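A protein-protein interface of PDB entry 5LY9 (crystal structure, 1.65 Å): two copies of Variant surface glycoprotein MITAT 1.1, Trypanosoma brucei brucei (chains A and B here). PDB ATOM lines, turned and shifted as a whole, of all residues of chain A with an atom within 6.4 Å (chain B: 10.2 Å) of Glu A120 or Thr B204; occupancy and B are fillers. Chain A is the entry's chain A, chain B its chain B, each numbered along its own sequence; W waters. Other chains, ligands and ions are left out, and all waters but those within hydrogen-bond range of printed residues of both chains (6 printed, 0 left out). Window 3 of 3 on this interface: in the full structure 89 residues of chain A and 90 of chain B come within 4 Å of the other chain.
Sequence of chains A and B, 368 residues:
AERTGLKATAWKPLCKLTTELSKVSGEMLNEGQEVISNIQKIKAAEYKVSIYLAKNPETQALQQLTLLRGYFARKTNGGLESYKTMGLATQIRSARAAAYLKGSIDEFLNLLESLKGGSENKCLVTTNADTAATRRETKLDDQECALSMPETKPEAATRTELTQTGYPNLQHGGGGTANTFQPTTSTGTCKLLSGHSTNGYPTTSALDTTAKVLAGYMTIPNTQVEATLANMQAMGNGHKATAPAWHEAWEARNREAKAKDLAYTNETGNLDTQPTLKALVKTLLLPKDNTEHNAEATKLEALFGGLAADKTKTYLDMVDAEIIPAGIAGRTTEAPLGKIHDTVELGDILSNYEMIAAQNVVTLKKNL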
ATOM      1  N   GLY A 117       0.631   2.591  21.860  1.00  0.00           N
ATOM      2  CA  GLY A 117       0.378   2.220  23.222  1.00  0.00           C
ATOM      3  C   GLY A 117       1.548   1.408  23.779  1.00  0.00           C
ATOM      4  O   GLY A 117       1.669   0.224  23.498  1.00  0.00           O
ATOM      5  N   GLY A 118       2.325   2.049  24.654  1.00  0.00           N
ATOM      6  CA  GLY A 118       3.527   1.376  25.226  1.00  0.00           C
ATOM      7  C   GLY A 118       4.460   0.794  24.168  1.00  0.00           C
ATOM      8  O   GLY A 118       4.483   1.278  23.043  1.00  0.00           O
ATOM      9  N   SER A 119       5.174  -0.282  24.527  1.00  0.00           N
ATOM     10  CA  SER A 119       6.119  -0.901  23.636  1.00  0.00           C
ATOM     11  C   SER A 119       5.413  -1.818  22.667  1.00  0.00           C
ATOM     12  O   SER A 119       5.972  -2.125  21.605  1.00  0.00           O
ATOM     13  CB  SER A 119       7.106  -1.732  24.471  1.00  0.00           C
ATOM     14  OG  SER A 119       6.409  -2.778  25.119  1.00  0.00           O
ATOM     15  N   GLU A 120       4.202  -2.260  22.988  1.00  0.00           N
ATOM     16  CA  GLU A 120       3.531  -3.340  22.218  1.00  0.00           C
ATOM     17  C   GLU A 120       2.631  -2.879  21.060  1.00  0.00           C
ATOM     18  O   GLU A 120       2.244  -3.719  20.259  1.00  0.00           O
ATOM     19  CB  GLU A 120       2.635  -4.184  23.125  1.00  0.00           C
ATOM     20  CG  GLU A 120       3.427  -4.756  24.322  1.00  0.00           C
ATOM     21  CD  GLU A 120       3.408  -3.876  25.573  1.00  0.00           C
ATOM     22  OE1 GLU A 120       2.933  -2.737  25.610  1.00  0.00           O
ATOM     23  OE2 GLU A 120       3.924  -4.394  26.606  1.00  0.00           O
ATOM     24  N   ASN A 121       2.311  -1.601  20.965  1.00  0.00           N
ATOM     25  CA  ASN A 121       1.367  -1.131  19.932  1.00  0.00           C
ATOM     26  C   ASN A 121       1.938   0.070  19.255  1.00  0.00           C
ATOM     27  O   ASN A 121       2.025   1.163  19.846  1.00  0.00           O
ATOM     28  CB  ASN A 121      -0.004  -0.828  20.545  1.00  0.00           C
ATOM     29  CG  ASN A 121      -0.527  -2.000  21.384  1.00  0.00           C
ATOM     30  OD1 ASN A 121      -1.189  -2.946  20.874  1.00  0.00           O
ATOM     31  ND2 ASN A 121      -0.217  -1.971  22.696  1.00  0.00           N
ATOM     32  N   LYS A 122       2.309  -0.115  17.983  1.00  0.00           N
ATOM     33  CA  LYS A 122       2.868   0.976  17.209  1.00  0.00           C
ATOM     34  C   LYS A 122       2.531   0.710  15.770  1.00  0.00           C
ATOM     35  O   LYS A 122       2.887  -0.336  15.254  1.00  0.00           O
ATOM     36  CB  LYS A 122       4.382   1.046  17.384  1.00  0.00           C
ATOM     37  CG  LYS A 122       4.867   1.213  18.787  1.00  0.00           C
ATOM     38  CD  LYS A 122       6.353   1.276  18.942  1.00  0.00           C
ATOM     39  CE  LYS A 122       6.589   1.646  20.405  1.00  0.00           C
ATOM     40  NZ  LYS A 122       8.022   1.457  20.728  1.00  0.00           N
ATOM     41  N   THR A 187       8.866  -6.428  19.121  1.00  0.00           N
ATOM     42  CA  THR A 187       7.958  -6.189  20.269  1.00  0.00           C
ATOM     43  C   THR A 187       6.703  -5.399  19.846  1.00  0.00           C
ATOM     44  O   THR A 187       5.587  -5.794  20.153  1.00  0.00           O
ATOM     45  CB  THR A 187       8.691  -5.477  21.418  1.00  0.00           C
ATOM     46  OG1 THR A 187       9.742  -6.350  21.808  1.00  0.00           O
ATOM     47  CG2 THR A 187       7.755  -5.227  22.598  1.00  0.00           C
ATOM     48  N   GLY A 188       6.894  -4.305  19.137  1.00  0.00           N
ATOM     49  CA  GLY A 188       5.736  -3.496  18.655  1.00  0.00           C
ATOM     50  C   GLY A 188       4.882  -4.239  17.652  1.00  0.00           C
ATOM     51  O   GLY A 188       5.362  -5.080  16.883  1.00  0.00           O
ATOM     52  N   THR A 189       3.593  -3.979  17.675  1.00  0.00           N
ATOM     53  CA  THR A 189       2.677  -4.638  16.738  1.00  0.00           C
ATOM     54  C   THR A 189       1.599  -3.625  16.353  1.00  0.00           C
ATOM     55  O   THR A 189       1.438  -2.632  17.017  1.00  0.00           O
ATOM     56  CB  THR A 189       1.928  -5.826  17.373  1.00  0.00           C
ATOM     57  OG1 THR A 189       1.068  -5.349  18.435  1.00  0.00           O
ATOM     58  CG2 THR A 189       2.842  -6.851  17.896  1.00  0.00           C
ATOM     59  N   CYS A 190       0.935  -3.839  15.223  1.00  0.00           N
ATOM     60  CA  CYS A 190      -0.227  -3.048  14.817  1.00  0.00           C
ATOM     61  C   CYS A 190      -1.250  -4.090  14.421  1.00  0.00           C
ATOM     62  O   CYS A 190      -1.293  -4.535  13.243  1.00  0.00           O
ATOM     63  CB  CYS A 190       0.185  -2.185  13.639  1.00  0.00           C
ATOM     64  SG  CYS A 190      -1.176  -1.111  13.086  1.00  0.00           S
ATOM     65  N   GLY B 195      -9.449   1.988  23.774  1.00  0.00           N
ATOM     66  CA  GLY B 195      -8.004   1.921  23.744  1.00  0.00           C
ATOM     67  C   GLY B 195      -7.419   1.419  25.068  1.00  0.00           C
ATOM     68  O   GLY B 195      -6.271   1.734  25.364  1.00  0.00           O
ATOM     69  N   HIS B 196      -8.199   0.679  25.849  1.00  0.00           N
ATOM     70  CA  HIS B 196      -7.705   0.060  27.079  1.00  0.00           C
ATOM     71  C   HIS B 196      -7.400  -1.391  26.791  1.00  0.00           C
ATOM     72  O   HIS B 196      -8.113  -2.043  26.082  1.00  0.00           O
ATOM     73  CB  HIS B 196      -8.723   0.252  28.222  1.00  0.00           C
ATOM     74  CG  HIS B 196      -8.184  -0.113  29.548  1.00  0.00           C
ATOM     75  ND1 HIS B 196      -8.249  -1.402  30.044  1.00  0.00           N
ATOM     76  CD2 HIS B 196      -7.512   0.623  30.461  1.00  0.00           C
ATOM     77  CE1 HIS B 196      -7.666  -1.430  31.234  1.00  0.00           C
ATOM     78  NE2 HIS B 196      -7.220  -0.219  31.508  1.00  0.00           N
ATOM     79  N   SER B 197      -6.329  -1.911  27.397  1.00  0.00           N
ATOM     80  CA  SER B 197      -5.796  -3.175  26.979  1.00  0.00           C
ATOM     81  C   SER B 197      -6.518  -4.415  27.512  1.00  0.00           C
ATOM     82  O   SER B 197      -6.372  -5.474  26.919  1.00  0.00           O
ATOM     83  CB  SER B 197      -4.334  -3.249  27.363  1.00  0.00           C
ATOM     84  OG  SER B 197      -4.208  -2.935  28.750  1.00  0.00           O
ATOM     85  N   THR B 198      -7.288  -4.343  28.595  1.00  0.00           N
ATOM     86  CA  THR B 198      -7.898  -5.612  29.053  1.00  0.00           C
ATOM     87  C   THR B 198      -9.020  -6.161  28.177  1.00  0.00           C
ATOM     88  O   THR B 198      -8.984  -7.324  27.854  1.00  0.00           O
ATOM     89  CB  THR B 198      -8.005  -5.787  30.583  1.00  0.00           C
ATOM     90  OG1 THR B 198      -9.253  -6.418  31.016  1.00  0.00           O
ATOM     91  CG2 THR B 198      -7.538  -4.696  31.349  1.00  0.00           C
ATOM     92  N   ASN B 199      -9.910  -5.287  27.680  1.00  0.00           N
ATOM     93  CA  ASN B 199     -11.030  -5.677  26.816  1.00  0.00           C
ATOM     94  C   ASN B 199     -11.010  -5.026  25.423  1.00  0.00           C
ATOM     95  O   ASN B 199     -11.691  -5.502  24.527  1.00  0.00           O
ATOM     96  CB  ASN B 199     -12.293  -5.207  27.488  1.00  0.00           C
ATOM     97  CG  ASN B 199     -12.481  -5.844  28.832  1.00  0.00           C
ATOM     98  OD1 ASN B 199     -12.229  -7.058  28.986  1.00  0.00           O
ATOM     99  ND2 ASN B 199     -12.915  -5.076  29.785  1.00  0.00           N
ATOM    100  N   GLY B 200     -10.170  -4.007  25.259  1.00  0.00           N
ATOM    101  CA  GLY B 200     -10.182  -3.230  24.034  1.00  0.00           C
ATOM    102  C   GLY B 200      -9.104  -3.626  23.065  1.00  0.00           C
ATOM    103  O   GLY B 200      -8.572  -4.754  23.049  1.00  0.00           O
ATOM    104  N   TYR B 201      -8.748  -2.665  22.232  1.00  0.00           N
ATOM    105  CA  TYR B 201      -7.821  -2.889  21.092  1.00  0.00           C
ATOM    106  C   TYR B 201      -6.426  -3.326  21.431  1.00  0.00           C
ATOM    107  O   TYR B 201      -5.943  -4.289  20.865  1.00  0.00           O
ATOM    108  CB  TYR B 201      -7.871  -1.678  20.128  1.00  0.00           C
ATOM    109  CG  TYR B 201      -6.786  -1.703  19.113  1.00  0.00           C
ATOM    110  CD1 TYR B 201      -6.914  -2.440  17.932  1.00  0.00           C
ATOM    111  CD2 TYR B 201      -5.578  -1.093  19.362  1.00  0.00           C
ATOM    112  CE1 TYR B 201      -5.887  -2.531  17.021  1.00  0.00           C
ATOM    113  CE2 TYR B 201      -4.531  -1.170  18.472  1.00  0.00           C
ATOM    114  CZ  TYR B 201      -4.665  -1.854  17.295  1.00  0.00           C
ATOM    115  OH  TYR B 201      -3.634  -1.897  16.434  1.00  0.00           O
ATOM    116  N   PRO B 202      -5.703  -2.544  22.270  1.00  0.00           N
ATOM    117  CA  PRO B 202      -4.278  -2.753  22.348  1.00  0.00           C
ATOM    118  C   PRO B 202      -3.813  -3.877  23.246  1.00  0.00           C
ATOM    119  O   PRO B 202      -4.539  -4.259  24.126  1.00  0.00           O
ATOM    120  CB  PRO B 202      -3.761  -1.436  22.885  1.00  0.00           C
ATOM    121  CG  PRO B 202      -4.819  -0.991  23.800  1.00  0.00           C
ATOM    122  CD  PRO B 202      -6.126  -1.419  23.132  1.00  0.00           C
ATOM    123  N   THR B 203      -2.697  -4.474  22.901  1.00  0.00           N
ATOM    124  CA  THR B 203      -2.131  -5.537  23.705  1.00  0.00           C
ATOM    125  C   THR B 203      -1.288  -4.973  24.857  1.00  0.00           C
ATOM    126  O   THR B 203      -0.412  -4.133  24.658  1.00  0.00           O
ATOM    127  CB  THR B 203      -1.195  -6.377  22.799  1.00  0.00           C
ATOM    128  OG1 THR B 203      -1.940  -6.879  21.659  1.00  0.00           O
ATOM    129  CG2 THR B 203      -0.560  -7.509  23.568  1.00  0.00           C
ATOM    130  N   THR B 204      -1.577  -5.441  26.077  1.00  0.00           N
ATOM    131  CA  THR B 204      -0.777  -5.249  27.291  1.00  0.00           C
ATOM    132  C   THR B 204      -0.826  -3.814  27.846  1.00  0.00           C
ATOM    133  O   THR B 204      -1.149  -3.611  29.011  1.00  0.00           O
ATOM    134  CB  THR B 204       0.651  -5.729  27.083  1.00  0.00           C
ATOM    135  OG1 THR B 204       0.619  -7.115  26.754  1.00  0.00           O
ATOM    136  CG2 THR B 204       1.495  -5.512  28.362  1.00  0.00           C
ATOM    137  N   SER B 205      -0.510  -2.827  27.025  1.00  0.00           N
ATOM    138  CA  SER B 205      -0.522  -1.413  27.468  1.00  0.00           C
ATOM    139  C   SER B 205      -1.680  -0.724  26.844  1.00  0.00           C
ATOM    140  O   SER B 205      -1.953  -0.950  25.689  1.00  0.00           O
ATOM    141  CB  SER B 205       0.714  -0.748  26.925  1.00  0.00           C
ATOM    142  OG  SER B 205       1.897  -1.346  27.448  1.00  0.00           O
ATOM    143  N   ALA B 206      -2.317   0.153  27.585  1.00  0.00           N
ATOM    144  CA  ALA B 206      -3.346   1.040  27.020  1.00  0.00           C
ATOM    145  C   ALA B 206      -2.736   1.983  26.003  1.00  0.00           C
ATOM    146  O   ALA B 206      -1.500   2.189  25.930  1.00  0.00           O
ATOM    147  CB  ALA B 206      -3.956   1.863  28.135  1.00  0.00           C
ATOM    148  N   LEU B 207      -3.589   2.579  25.156  1.00  0.00           N
ATOM    149  CA  LEU B 207      -3.081   3.639  24.315  1.00  0.00           C
ATOM    150  C   LEU B 207      -2.457   4.764  25.154  1.00  0.00           C
ATOM    151  O   LEU B 207      -2.959   5.106  26.201  1.00  0.00           O
ATOM    152  CB  LEU B 207      -4.146   4.230  23.366  1.00  0.00           C
ATOM    153  CG  LEU B 207      -4.810   3.252  22.426  1.00  0.00           C
ATOM    154  CD1 LEU B 207      -5.813   3.983  21.557  1.00  0.00           C
ATOM    155  CD2 LEU B 207      -3.792   2.532  21.598  1.00  0.00           C
ATOM    156  N   ASP B 208      -1.408   5.380  24.640  1.00  0.00           N
ATOM    157  CA  ASP B 208      -0.698   6.410  25.404  1.00  0.00           C
ATOM    158  C   ASP B 208      -1.595   7.630  25.716  1.00  0.00           C
ATOM    159  O   ASP B 208      -1.560   8.199  26.831  1.00  0.00           O
ATOM    160  CB  ASP B 208       0.556   6.801  24.670  1.00  0.00           C
ATOM    161  CG  ASP B 208       1.565   5.691  24.554  1.00  0.00           C
ATOM    162  OD1 ASP B 208       1.556   4.693  25.324  1.00  0.00           O
ATOM    163  OD2 ASP B 208       2.386   5.834  23.653  1.00  0.00           O
ATOM    164  N   ASN B 222      -8.757   5.690  26.467  1.00  0.00           N
ATOM    165  CA  ASN B 222      -7.744   4.776  26.907  1.00  0.00           C
ATOM    166  C   ASN B 222      -7.999   4.222  28.338  1.00  0.00           C
ATOM    167  O   ASN B 222      -7.077   3.766  28.979  1.00  0.00           O
ATOM    168  CB  ASN B 222      -6.358   5.368  26.753  1.00  0.00           C
ATOM    169  CG  ASN B 222      -6.080   6.491  27.710  1.00  0.00           C
ATOM    170  OD1 ASN B 222      -6.974   6.981  28.352  1.00  0.00           O
ATOM    171  ND2 ASN B 222      -4.829   6.933  27.739  1.00  0.00           N
HETATM  172  O   HOH W   1      -1.275  -3.641  18.284  1.00  0.00           O
HETATM  173  O   HOH W   2       4.518  -2.921  28.740  1.00  0.00           O
HETATM  174  O   HOH W   3      -1.366  -0.800  17.430  1.00  0.00           O
HETATM  175  O   HOH W   4       5.263  -0.930  27.370  1.00  0.00           O
HETATM  176  O   HOH W   5      -0.042  -7.616  19.854  1.00  0.00           O
HETATM  177  O   HOH W   6       4.402   4.131  22.735  1.00  0.00           O
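No position is printed for both chains.
Of the 13 pairs that touch across the chains among the printed residues, none has its exchanged pair printed and touching as well.
CB of Ser B205 touches O of Gly A117, at 3.7 Å.
Ala B206 touches Gly A117.
Leu B207 touches Gly A117.
Asp B208 touches Gly A117.
Gly A118 touches Ser B205.
Thr B203 touches Glu A120.
Thr B204 touches Glu A120.
CA of Pro B202 touches OD1 of Asn A121, 3.4 Å away.
Asn A121 touches Ser B205.
Cys A190 touches Tyr B201.
N of Gly A118 sits at hydrogen-bond distance from OD1 of Asp B208, at 2.8 Å.
The side-chain hydroxyl of Ser B205 lies within hydrogen-bond range of the side-chain carboxylate of Glu A120, at 2.5 Å.
The side-chain amide nitrogen (ND2) of Asn A121 is in hydrogen-bond range of the backbone carbonyl oxygen (O) of Thr B203, 2.9 Å away.
Gly A117 touches just these residues of chain B: Ser B205 (3.7 Å), Ala B206 (3.3 Å), Leu B207 (3.9 Å) and Asp B208 (3.5 Å).
Gly A118 touches just these residues of chain B: Ser B205 and Asp B208.
Printed residues of chain B within 4 Å of Glu A120: Thr B203, Thr B204 and Ser B205.
Of the printed residues of chain B, Asn A121 touches Pro B202 (3.4 Å), Thr B203 (2.9 Å) and Ser B205 (3.6 Å).
Lys A122 touches none of the printed residues of chain B.
No residue of chain B comes within 4 Å of Thr A189.
Of the printed residues of chain B, Cys A190 touches Tyr B201.
Of the printed residues of chain A, Pro B202 touches Asn A121.
Of the printed residues of chain A, Thr B203 touches Glu A120 (3.4 Å) and Asn A121 (2.9 Å).
Of chain A, only Glu A120 comes within 4 Å of Thr B204.
Of the printed residues of chain A, Ala B206 touches Gly A117.
Of the printed residues of chain A, Leu B207 touches Gly A117.
Of the 15 printed residues of chain B, 8 touch a printed residue of chain A.
Hydrophobic or aromatic side chains of chain B that line the printed part of chain A: Tyr B201 and Pro B202.
Printed residues of chain A that touch a printed residue of chain B: Gly A117, Gly A118, Glu A120, Asn A121 and Cys A190.
Among the printed residues, no Asp or Glu carboxylate lies within 4 Å of a Lys or Arg side-chain nitrogen of the other chain.
Water W2 bridges OE2 of Glu A120 (2.7 Å) and OG of Ser B205 (3.3 Å).
Water W1 lies within hydrogen-bond range of OD1 of Asn A121 (2.7 Å), OG1 of Thr A189 (2.9 Å) and OH of Tyr B201 (3.5 Å).
Water W3 lies within hydrogen-bond range of OH of Tyr B201 and O of Thr A189.
Water W5 bridges the side-chain hydroxyl of Thr B203 (2.7 Å) and the side-chain hydroxyl of Thr A189 (2.9 Å).
Water W6 bridges OD2 of Asp B208 and O of Gly A118.
Water W4 lies within hydrogen-bond range of N of Ser A119 (2.9 Å), OG of Ser B205 (3.4 Å) and OE1 of Glu A120 (3.4 Å).
The backbone carbonyl oxygen (O) of Gly A117 is in hydrogen-bond range of the side-chain amide nitrogen (ND2) of Asn A121, at 3.0 Å.
The side-chain carboxylate (OE2) of Glu A120 sits close to the side-chain hydroxyl (OG) of Ser A119 (3.3 Å).
The backbone carbonyl oxygen of Glu A120 sits at hydrogen-bond distance from the side-chain hydroxyl of Thr A189 (2.7 Å).
The backbone NH (N) of Leu B207 sits at hydrogen-bond distance from the backbone carbonyl oxygen (O) of Gly B195 (2.8 Å).
O of Thr B204 is in hydrogen-bond range of OG of Ser B197 (3.1 Å).
O of Leu B207 lies within hydrogen-bond range of ND2 of Asn B222 (3.0 Å).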
